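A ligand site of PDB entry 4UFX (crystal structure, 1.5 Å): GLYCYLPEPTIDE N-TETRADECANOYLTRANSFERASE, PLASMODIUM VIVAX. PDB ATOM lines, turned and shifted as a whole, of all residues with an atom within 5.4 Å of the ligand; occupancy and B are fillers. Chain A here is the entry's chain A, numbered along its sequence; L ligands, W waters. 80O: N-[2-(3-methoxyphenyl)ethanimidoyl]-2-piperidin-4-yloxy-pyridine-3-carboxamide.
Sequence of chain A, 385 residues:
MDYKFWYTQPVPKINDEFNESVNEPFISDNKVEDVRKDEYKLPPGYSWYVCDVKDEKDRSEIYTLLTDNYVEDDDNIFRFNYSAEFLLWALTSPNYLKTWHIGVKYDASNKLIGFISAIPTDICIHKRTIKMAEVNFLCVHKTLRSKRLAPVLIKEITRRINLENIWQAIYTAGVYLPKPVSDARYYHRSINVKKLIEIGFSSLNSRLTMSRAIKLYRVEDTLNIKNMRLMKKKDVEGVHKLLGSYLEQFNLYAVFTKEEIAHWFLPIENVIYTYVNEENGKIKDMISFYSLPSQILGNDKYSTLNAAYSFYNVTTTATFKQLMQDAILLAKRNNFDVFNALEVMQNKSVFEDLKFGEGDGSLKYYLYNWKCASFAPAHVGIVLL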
ATOM      1  N   VAL A  71      -8.429  16.711  17.299  1.00  0.00           N
ATOM      2  CA  VAL A  71      -8.222  15.912  18.552  1.00  0.00           C
ATOM      3  C   VAL A  71      -8.986  14.584  18.542  1.00  0.00           C
ATOM      4  O   VAL A  71     -10.193  14.570  18.216  1.00  0.00           O
ATOM      5  CB  VAL A  71      -8.791  16.788  19.747  1.00  0.00           C
ATOM      6  CG1 VAL A  71      -8.550  16.108  21.094  1.00  0.00           C
ATOM      7  CG2 VAL A  71      -8.018  18.118  19.755  1.00  0.00           C
ATOM      8  N   GLU A  72      -8.237  13.525  18.949  1.00  0.00           N
ATOM      9  CA  GLU A  72      -8.870  12.219  19.186  1.00  0.00           C
ATOM     10  C   GLU A  72      -9.004  11.953  20.644  1.00  0.00           C
ATOM     11  O   GLU A  72      -8.237  12.534  21.446  1.00  0.00           O
ATOM     12  CB  GLU A  72      -8.064  11.116  18.465  1.00  0.00           C
ATOM     13  CG  GLU A  72      -8.234  11.294  16.956  1.00  0.00           C
ATOM     14  CD  GLU A  72      -7.350  10.381  16.121  1.00  0.00           C
ATOM     15  OE1 GLU A  72      -6.789   9.428  16.745  1.00  0.00           O
ATOM     16  OE2 GLU A  72      -7.254  10.570  14.892  1.00  0.00           O
ATOM     17  N   ASP A  73      -9.917  11.056  21.047  1.00  0.00           N
ATOM     18  CA  ASP A  73      -9.943  10.656  22.479  1.00  0.00           C
ATOM     19  C   ASP A  73      -8.733   9.791  22.797  1.00  0.00           C
ATOM     20  O   ASP A  73      -8.080   9.303  21.878  1.00  0.00           O
ATOM     21  CB  ASP A  73     -11.241   9.914  22.816  1.00  0.00           C
ATOM     22  CG  ASP A  73     -11.367   8.577  22.090  1.00  0.00           C
ATOM     23  OD1 ASP A  73     -11.135   8.486  20.903  1.00  0.00           O
ATOM     24  OD2 ASP A  73     -11.786   7.628  22.790  1.00  0.00           O
ATOM     25  N   PHE A  78     -12.610   8.080  18.575  1.00  0.00           N
ATOM     26  CA  PHE A  78     -13.472   9.235  18.134  1.00  0.00           C
ATOM     27  C   PHE A  78     -12.530  10.365  17.776  1.00  0.00           C
ATOM     28  O   PHE A  78     -11.457  10.506  18.402  1.00  0.00           O
ATOM     29  CB  PHE A  78     -14.317   9.743  19.407  1.00  0.00           C
ATOM     30  CG  PHE A  78     -15.236   8.702  19.921  1.00  0.00           C
ATOM     31  CD1 PHE A  78     -16.292   8.220  19.104  1.00  0.00           C
ATOM     32  CD2 PHE A  78     -15.042   8.160  21.146  1.00  0.00           C
ATOM     33  CE1 PHE A  78     -17.051   7.148  19.496  1.00  0.00           C
ATOM     34  CE2 PHE A  78     -15.815   7.078  21.562  1.00  0.00           C
ATOM     35  CZ  PHE A  78     -16.832   6.547  20.726  1.00  0.00           C
ATOM     36  N   ARG A  79     -12.916  11.230  16.842  1.00  0.00           N
ATOM     37  CA  ARG A  79     -12.166  12.535  16.611  1.00  0.00           C
ATOM     38  C   ARG A  79     -13.212  13.633  16.578  1.00  0.00           C
ATOM     39  O   ARG A  79     -14.313  13.508  15.992  1.00  0.00           O
ATOM     40  CB  ARG A  79     -11.544  12.473  15.216  1.00  0.00           C
ATOM     41  CG  ARG A  79     -10.505  13.601  15.069  1.00  0.00           C
ATOM     42  CD  ARG A  79      -9.781  13.557  13.732  1.00  0.00           C
ATOM     43  NE  ARG A  79      -9.145  12.263  13.490  1.00  0.00           N
ATOM     44  CZ  ARG A  79      -9.419  11.416  12.451  1.00  0.00           C
ATOM     45  NH1 ARG A  79     -10.257  11.694  11.413  1.00  0.00           N
ATOM     46  NH2 ARG A  79      -8.764  10.270  12.463  1.00  0.00           N
ATOM     47  N   PHE A  80     -12.901  14.715  17.306  1.00  0.00           N
ATOM     48  CA  PHE A  80     -13.893  15.832  17.254  1.00  0.00           C
ATOM     49  C   PHE A  80     -14.155  16.244  15.812  1.00  0.00           C
ATOM     50  O   PHE A  80     -13.250  16.252  14.942  1.00  0.00           O
ATOM     51  CB  PHE A  80     -13.325  17.054  17.959  1.00  0.00           C
ATOM     52  CG  PHE A  80     -13.295  16.966  19.453  1.00  0.00           C
ATOM     53  CD1 PHE A  80     -14.377  16.435  20.146  1.00  0.00           C
ATOM     54  CD2 PHE A  80     -12.261  17.571  20.150  1.00  0.00           C
ATOM     55  CE1 PHE A  80     -14.399  16.413  21.567  1.00  0.00           C
ATOM     56  CE2 PHE A  80     -12.224  17.549  21.545  1.00  0.00           C
ATOM     57  CZ  PHE A  80     -13.275  16.973  22.242  1.00  0.00           C
ATOM     58  N   TYR A  82     -15.993  19.394  14.667  1.00  0.00           N
ATOM     59  CA  TYR A  82     -16.646  20.664  14.654  1.00  0.00           C
ATOM     60  C   TYR A  82     -17.249  20.998  13.299  1.00  0.00           C
ATOM     61  O   TYR A  82     -16.597  20.776  12.270  1.00  0.00           O
ATOM     62  CB  TYR A  82     -15.646  21.798  14.927  1.00  0.00           C
ATOM     63  CG  TYR A  82     -15.091  21.817  16.341  1.00  0.00           C
ATOM     64  CD1 TYR A  82     -13.966  21.079  16.696  1.00  0.00           C
ATOM     65  CD2 TYR A  82     -15.743  22.577  17.364  1.00  0.00           C
ATOM     66  CE1 TYR A  82     -13.503  21.089  18.013  1.00  0.00           C
ATOM     67  CE2 TYR A  82     -15.234  22.591  18.650  1.00  0.00           C
ATOM     68  CZ  TYR A  82     -14.139  21.880  18.945  1.00  0.00           C
ATOM     69  OH  TYR A  82     -13.618  21.976  20.230  1.00  0.00           O
ATOM     70  N   ASN A 136      -7.582  28.624  20.121  1.00  0.00           N
ATOM     71  CA  ASN A 136      -8.231  27.319  19.885  1.00  0.00           C
ATOM     72  C   ASN A 136      -7.942  26.866  18.472  1.00  0.00           C
ATOM     73  O   ASN A 136      -7.431  27.617  17.638  1.00  0.00           O
ATOM     74  CB  ASN A 136      -9.730  27.451  20.126  1.00  0.00           C
ATOM     75  CG  ASN A 136     -10.387  26.150  20.606  1.00  0.00           C
ATOM     76  OD1 ASN A 136      -9.808  25.088  20.598  1.00  0.00           O
ATOM     77  ND2 ASN A 136     -11.651  26.299  21.132  1.00  0.00           N
ATOM     78  N   THR A 172      -7.216  25.839  26.526  1.00  0.00           N
ATOM     79  CA  THR A 172      -7.345  24.551  27.234  1.00  0.00           C
ATOM     80  C   THR A 172      -6.680  23.486  26.437  1.00  0.00           C
ATOM     81  O   THR A 172      -6.434  23.607  25.197  1.00  0.00           O
ATOM     82  CB  THR A 172      -8.806  24.096  27.462  1.00  0.00           C
ATOM     83  OG1 THR A 172      -9.503  24.002  26.182  1.00  0.00           O
ATOM     84  CG2 THR A 172      -9.600  25.045  28.364  1.00  0.00           C
ATOM     85  N   TYR A 186     -13.860  15.452  33.089  1.00  0.00           N
ATOM     86  CA  TYR A 186     -15.139  15.471  32.356  1.00  0.00           C
ATOM     87  C   TYR A 186     -15.972  14.243  32.678  1.00  0.00           C
ATOM     88  O   TYR A 186     -15.450  13.174  33.086  1.00  0.00           O
ATOM     89  CB  TYR A 186     -14.937  15.650  30.875  1.00  0.00           C
ATOM     90  CG  TYR A 186     -13.719  15.016  30.238  1.00  0.00           C
ATOM     91  CD1 TYR A 186     -13.756  13.685  29.848  1.00  0.00           C
ATOM     92  CD2 TYR A 186     -12.529  15.792  29.977  1.00  0.00           C
ATOM     93  CE1 TYR A 186     -12.680  13.105  29.192  1.00  0.00           C
ATOM     94  CE2 TYR A 186     -11.471  15.230  29.360  1.00  0.00           C
ATOM     95  CZ  TYR A 186     -11.523  13.881  28.974  1.00  0.00           C
ATOM     96  OH  TYR A 186     -10.419  13.358  28.316  1.00  0.00           O
ATOM     97  N   TYR A 187     -17.258  14.438  32.505  1.00  0.00           N
ATOM     98  CA  TYR A 187     -18.300  13.436  32.824  1.00  0.00           C
ATOM     99  C   TYR A 187     -19.317  13.488  31.683  1.00  0.00           C
ATOM    100  O   TYR A 187     -19.441  14.498  30.956  1.00  0.00           O
ATOM    101  CB  TYR A 187     -19.048  13.838  34.142  1.00  0.00           C
ATOM    102  CG  TYR A 187     -18.199  13.654  35.389  1.00  0.00           C
ATOM    103  CD1 TYR A 187     -17.135  14.528  35.680  1.00  0.00           C
ATOM    104  CD2 TYR A 187     -18.495  12.621  36.286  1.00  0.00           C
ATOM    105  CE1 TYR A 187     -16.371  14.359  36.834  1.00  0.00           C
ATOM    106  CE2 TYR A 187     -17.718  12.441  37.438  1.00  0.00           C
ATOM    107  CZ  TYR A 187     -16.709  13.314  37.668  1.00  0.00           C
ATOM    108  OH  TYR A 187     -15.976  13.094  38.817  1.00  0.00           O
ATOM    109  N   PHE A 201     -18.698   3.670  23.140  1.00  0.00           N
ATOM    110  CA  PHE A 201     -18.529   4.810  24.051  1.00  0.00           C
ATOM    111  C   PHE A 201     -18.823   4.368  25.502  1.00  0.00           C
ATOM    112  O   PHE A 201     -18.244   4.944  26.448  1.00  0.00           O
ATOM    113  CB  PHE A 201     -19.492   5.941  23.602  1.00  0.00           C
ATOM    114  CG  PHE A 201     -19.423   7.186  24.454  1.00  0.00           C
ATOM    115  CD1 PHE A 201     -20.093   7.270  25.691  1.00  0.00           C
ATOM    116  CD2 PHE A 201     -18.712   8.275  23.999  1.00  0.00           C
ATOM    117  CE1 PHE A 201     -20.028   8.434  26.483  1.00  0.00           C
ATOM    118  CE2 PHE A 201     -18.652   9.444  24.770  1.00  0.00           C
ATOM    119  CZ  PHE A 201     -19.314   9.501  26.022  1.00  0.00           C
ATOM    120  N   TYR A 290     -23.617  23.550  23.733  1.00  0.00           N
ATOM    121  CA  TYR A 290     -23.223  23.623  22.301  1.00  0.00           C
ATOM    122  C   TYR A 290     -23.116  22.241  21.692  1.00  0.00           C
ATOM    123  O   TYR A 290     -22.965  21.258  22.376  1.00  0.00           O
ATOM    124  CB  TYR A 290     -21.882  24.457  22.072  1.00  0.00           C
ATOM    125  CG  TYR A 290     -20.660  24.024  22.822  1.00  0.00           C
ATOM    126  CD1 TYR A 290     -19.802  23.046  22.292  1.00  0.00           C
ATOM    127  CD2 TYR A 290     -20.231  24.714  23.978  1.00  0.00           C
ATOM    128  CE1 TYR A 290     -18.628  22.673  22.931  1.00  0.00           C
ATOM    129  CE2 TYR A 290     -19.021  24.349  24.596  1.00  0.00           C
ATOM    130  CZ  TYR A 290     -18.216  23.351  24.041  1.00  0.00           C
ATOM    131  OH  TYR A 290     -17.003  22.972  24.660  1.00  0.00           O
ATOM    132  N   LEU A 292     -21.083  19.547  19.528  1.00  0.00           N
ATOM    133  CA  LEU A 292     -19.707  19.171  19.031  1.00  0.00           C
ATOM    134  C   LEU A 292     -19.791  17.656  18.763  1.00  0.00           C
ATOM    135  O   LEU A 292     -19.570  16.869  19.695  1.00  0.00           O
ATOM    136  CB  LEU A 292     -18.634  19.603  20.078  1.00  0.00           C
ATOM    137  CG  LEU A 292     -17.237  19.060  19.747  1.00  0.00           C
ATOM    138  CD1 LEU A 292     -16.832  19.244  18.284  1.00  0.00           C
ATOM    139  CD2 LEU A 292     -16.265  19.686  20.773  1.00  0.00           C
ATOM    140  N   SER A 294     -18.614  13.991  17.392  1.00  0.00           N
ATOM    141  CA  SER A 294     -17.309  13.275  17.083  1.00  0.00           C
ATOM    142  C   SER A 294     -17.534  12.328  15.918  1.00  0.00           C
ATOM    143  O   SER A 294     -18.548  11.695  15.782  1.00  0.00           O
ATOM    144  CB  SER A 294     -16.857  12.518  18.300  1.00  0.00           C
ATOM    145  OG  SER A 294     -16.423  13.481  19.279  1.00  0.00           O
ATOM    146  N   LEU A 305     -21.201  10.681  16.301  1.00  0.00           N
ATOM    147  CA  LEU A 305     -21.758  10.751  17.661  1.00  0.00           C
ATOM    148  C   LEU A 305     -22.246  12.186  17.815  1.00  0.00           C
ATOM    149  O   LEU A 305     -21.428  13.110  17.689  1.00  0.00           O
ATOM    150  CB  LEU A 305     -20.612  10.487  18.638  1.00  0.00           C
ATOM    151  CG  LEU A 305     -20.984  10.834  20.089  1.00  0.00           C
ATOM    152  CD1 LEU A 305     -22.029   9.900  20.570  1.00  0.00           C
ATOM    153  CD2 LEU A 305     -19.764  10.556  20.952  1.00  0.00           C
ATOM    154  N   TYR A 309     -22.590  19.735  24.726  1.00  0.00           N
ATOM    155  CA  TYR A 309     -21.615  20.086  25.812  1.00  0.00           C
ATOM    156  C   TYR A 309     -22.204  21.220  26.597  1.00  0.00           C
ATOM    157  O   TYR A 309     -22.534  22.287  26.051  1.00  0.00           O
ATOM    158  CB  TYR A 309     -20.293  20.574  25.162  1.00  0.00           C
ATOM    159  CG  TYR A 309     -19.517  19.395  24.668  1.00  0.00           C
ATOM    160  CD1 TYR A 309     -19.870  18.716  23.489  1.00  0.00           C
ATOM    161  CD2 TYR A 309     -18.367  18.916  25.377  1.00  0.00           C
ATOM    162  CE1 TYR A 309     -19.115  17.636  23.051  1.00  0.00           C
ATOM    163  CE2 TYR A 309     -17.572  17.880  24.878  1.00  0.00           C
ATOM    164  CZ  TYR A 309     -18.039  17.191  23.793  1.00  0.00           C
ATOM    165  OH  TYR A 309     -17.265  16.078  23.361  1.00  0.00           O
ATOM    166  N   ASN A 340     -22.370  16.139  27.747  1.00  0.00           N
ATOM    167  CA  ASN A 340     -21.044  16.165  28.403  1.00  0.00           C
ATOM    168  C   ASN A 340     -20.893  17.416  29.252  1.00  0.00           C
ATOM    169  O   ASN A 340     -21.449  18.471  28.960  1.00  0.00           O
ATOM    170  CB  ASN A 340     -19.968  16.259  27.299  1.00  0.00           C
ATOM    171  CG  ASN A 340     -19.864  14.982  26.488  1.00  0.00           C
ATOM    172  OD1 ASN A 340     -19.511  13.934  27.014  1.00  0.00           O
ATOM    173  ND2 ASN A 340     -20.190  15.063  25.225  1.00  0.00           N
ATOM    174  N   ALA A 341     -20.105  17.266  30.343  1.00  0.00           N
ATOM    175  CA  ALA A 341     -19.861  18.465  31.177  1.00  0.00           C
ATOM    176  C   ALA A 341     -18.558  18.291  31.902  1.00  0.00           C
ATOM    177  O   ALA A 341     -18.025  17.183  31.971  1.00  0.00           O
ATOM    178  CB  ALA A 341     -21.002  18.637  32.169  1.00  0.00           C
ATOM    179  N   LEU A 342     -18.073  19.382  32.465  1.00  0.00           N
ATOM    180  CA  LEU A 342     -16.866  19.412  33.260  1.00  0.00           C
ATOM    181  C   LEU A 342     -17.221  19.676  34.698  1.00  0.00           C
ATOM    182  O   LEU A 342     -18.273  20.306  35.022  1.00  0.00           O
ATOM    183  CB  LEU A 342     -15.965  20.545  32.808  1.00  0.00           C
ATOM    184  CG  LEU A 342     -15.424  20.304  31.383  1.00  0.00           C
ATOM    185  CD1 LEU A 342     -14.982  21.630  30.705  1.00  0.00           C
ATOM    186  CD2 LEU A 342     -14.209  19.398  31.378  1.00  0.00           C
ATOM    187  N   LEU A 363      -9.634  18.077  31.408  1.00  0.00           N
ATOM    188  CA  LEU A 363      -9.284  19.240  30.564  1.00  0.00           C
ATOM    189  C   LEU A 363      -8.544  20.208  31.461  1.00  0.00           C
ATOM    190  O   LEU A 363      -9.012  20.620  32.529  1.00  0.00           O
ATOM    191  CB  LEU A 363     -10.617  19.869  30.097  1.00  0.00           C
ATOM    192  CG  LEU A 363     -10.347  20.900  29.025  1.00  0.00           C
ATOM    193  CD1 LEU A 363      -9.822  20.315  27.689  1.00  0.00           C
ATOM    194  CD2 LEU A 363     -11.621  21.716  28.845  1.00  0.00           C
ATOM    195  N   LEU A 384     -14.758  26.811  27.596  1.00  0.00           N
ATOM    196  CA  LEU A 384     -14.267  27.133  26.252  1.00  0.00           C
ATOM    197  C   LEU A 384     -14.806  26.122  25.217  1.00  0.00           C
ATOM    198  O   LEU A 384     -15.526  25.109  25.561  1.00  0.00           O
ATOM    199  CB  LEU A 384     -12.719  27.244  26.311  1.00  0.00           C
ATOM    200  CG  LEU A 384     -12.252  28.417  27.183  1.00  0.00           C
ATOM    201  CD1 LEU A 384     -10.745  28.563  27.334  1.00  0.00           C
ATOM    202  CD2 LEU A 384     -12.735  29.769  26.720  1.00  0.00           C
ATOM    203  N   LEU A 385     -14.493  26.403  23.925  1.00  0.00           N
ATOM    204  CA  LEU A 385     -15.099  25.601  22.854  1.00  0.00           C
ATOM    205  C   LEU A 385     -14.223  24.404  22.414  1.00  0.00           C
ATOM    206  O   LEU A 385     -13.048  24.244  22.794  1.00  0.00           O
ATOM    207  CB  LEU A 385     -15.420  26.499  21.667  1.00  0.00           C
ATOM    208  CG  LEU A 385     -16.253  27.705  22.069  1.00  0.00           C
ATOM    209  CD1 LEU A 385     -16.512  28.455  20.764  1.00  0.00           C
ATOM    210  CD2 LEU A 385     -17.590  27.366  22.662  1.00  0.00           C
ATOM    211  OXT LEU A 385     -14.910  23.512  21.805  1.00  0.00           O
HETATM  212  C   80O L   1     -16.128  11.498  22.491  1.00  0.00           C
HETATM  213  O   80O L   1     -15.261  12.076  21.519  1.00  0.00           O
HETATM  214  C1  80O L   1     -14.040  12.675  21.905  1.00  0.00           C
HETATM  215  C19 80O L   1     -13.721  12.769  23.274  1.00  0.00           C
HETATM  216  C5  80O L   1     -12.544  13.401  23.638  1.00  0.00           C
HETATM  217  C4  80O L   1     -11.682  13.883  22.637  1.00  0.00           C
HETATM  218  C3  80O L   1     -11.963  13.813  21.274  1.00  0.00           C
HETATM  219  C2  80O L   1     -13.126  13.147  20.888  1.00  0.00           C
HETATM  220  C6  80O L   1     -12.192  13.549  25.126  1.00  0.00           C
HETATM  221  C7  80O L   1     -12.180  15.020  25.556  1.00  0.00           C
HETATM  222  N1  80O L   1     -13.284  15.639  25.919  1.00  0.00           N
HETATM  223  C8  80O L   1     -13.077  16.936  26.234  1.00  0.00           C
HETATM  224  O1  80O L   1     -12.014  17.517  26.047  1.00  0.00           O
HETATM  225  N   80O L   1     -11.016  15.612  25.463  1.00  0.00           N
HETATM  226  C9  80O L   1     -14.244  17.589  26.882  1.00  0.00           C
HETATM  227  C13 80O L   1     -14.533  18.954  26.561  1.00  0.00           C
HETATM  228  N2  80O L   1     -15.507  19.580  27.201  1.00  0.00           N
HETATM  229  C12 80O L   1     -16.317  18.949  28.086  1.00  0.00           C
HETATM  230  C11 80O L   1     -16.105  17.603  28.414  1.00  0.00           C
HETATM  231  C10 80O L   1     -15.028  16.937  27.821  1.00  0.00           C
HETATM  232  O2  80O L   1     -13.781  19.599  25.614  1.00  0.00           O
HETATM  233  C14 80O L   1     -14.393  20.794  24.963  1.00  0.00           C
HETATM  234  C18 80O L   1     -13.698  22.022  25.534  1.00  0.00           C
HETATM  235  C17 80O L   1     -12.181  22.060  25.214  1.00  0.00           C
HETATM  236  N3  80O L   1     -12.037  21.870  23.747  1.00  0.00           N
HETATM  237  C16 80O L   1     -12.662  20.673  23.146  1.00  0.00           C
HETATM  238  C15 80O L   1     -14.144  20.592  23.483  1.00  0.00           C
HETATM  239  O   HOH W   1     -15.871  14.766  25.361  1.00  0.00           O
HETATM  240  O   HOH W   2      -8.777  16.803  24.913  1.00  0.00           O
HETATM  241  O   HOH W   3      -9.040  21.727  24.240  1.00  0.00           O
HETATM  242  O   HOH W   4     -17.410  12.555  25.524  1.00  0.00           O
HETATM  243  O   HOH W   5     -13.545  10.702  26.276  1.00  0.00           O
HETATM  244  O   HOH W   6     -10.870  22.516  20.741  1.00  0.00           O
HETATM  245  O   HOH W   7     -10.578  10.718  26.302  1.00  0.00           O
HETATM  246  O   HOH W   8     -16.352  22.337  27.505  1.00  0.00           O
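The chain-end carboxylate of Leu 385 lies within salt-bridge range of a nitrogen (N3) of the ligand (2.8 Å). The side-chain hydroxyl (OG) of Ser 294 is in hydrogen-bond range of an oxygen (O) of the ligand.
The chain-end carboxylate of Leu 385 is in hydrogen-bond range of the side-chain hydroxyl of Tyr 82 (2.6 Å). The side-chain amide nitrogen (ND2) of Asn 136 sits at hydrogen-bond distance from the chain-end carboxylate (O) of Leu 385, 3.0 Å away. N of Leu 305 lies within hydrogen-bond range of O of Ser 294 (2.9 Å). The backbone NH of Phe 78 sits at hydrogen-bond distance from the side-chain carboxylate of Asp 73 (2.8 Å). O of Tyr 290 sits at hydrogen-bond distance from N of Tyr 309 (2.8 Å). The side-chain hydroxyl (OH) of Tyr 290 is in hydrogen-bond range of the backbone carbonyl oxygen (O) of Leu 384 (2.7 Å). N of Phe 80 lies within hydrogen-bond range of O of Val 71 (2.9 Å). NH2 of Arg 79 lies within salt-bridge range of OE2 of Glu 72, at 2.9 Å.
Merely in contact with the ligand: Val 71 (3.6 Å), Glu 72 (3.6 Å), Asp 73 (3.4 Å), Phe 78 (3.3 Å), Phe 80 (3.5 Å), Tyr 82 (3.3 Å), Thr 172 (3.4 Å), Tyr 186 (3.3 Å), Phe 201 (3.97 Å), Tyr 290 (3.4 Å), Leu 292 (3.6 Å), Tyr 309 (3.4 Å), Leu 342 (3.7 Å), Leu 363 (3.7 Å) and Leu 384 (3.6 Å). Within 4 Å of the ligand: Val 71, Glu 72, Asp 73, Phe 78, Phe 80, Tyr 82, Thr 172, Tyr 186, Phe 201, Tyr 290, Leu 292, Ser 294, Tyr 309, Leu 342, Leu 363, Leu 384 and Leu 385. The nearest printed residue that does not touch the ligand is Leu 305 (4.1 Å).
Water W1 bridges OH of Tyr 309 and N1 of the ligand. Water W8 lies within hydrogen-bond range of N2 of the ligand (2.9 Å), OH of Tyr 290 (3.0 Å) and O of Leu 384 (3.5 Å). Water W3 bridges OG1 of Thr 172 (3.0 Å) and N3 of the ligand (3.0 Å). Water W6 lies within hydrogen-bond range of OD1 of Asn 136, OH of Tyr 82, N3 of the ligand and O of Leu 385.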
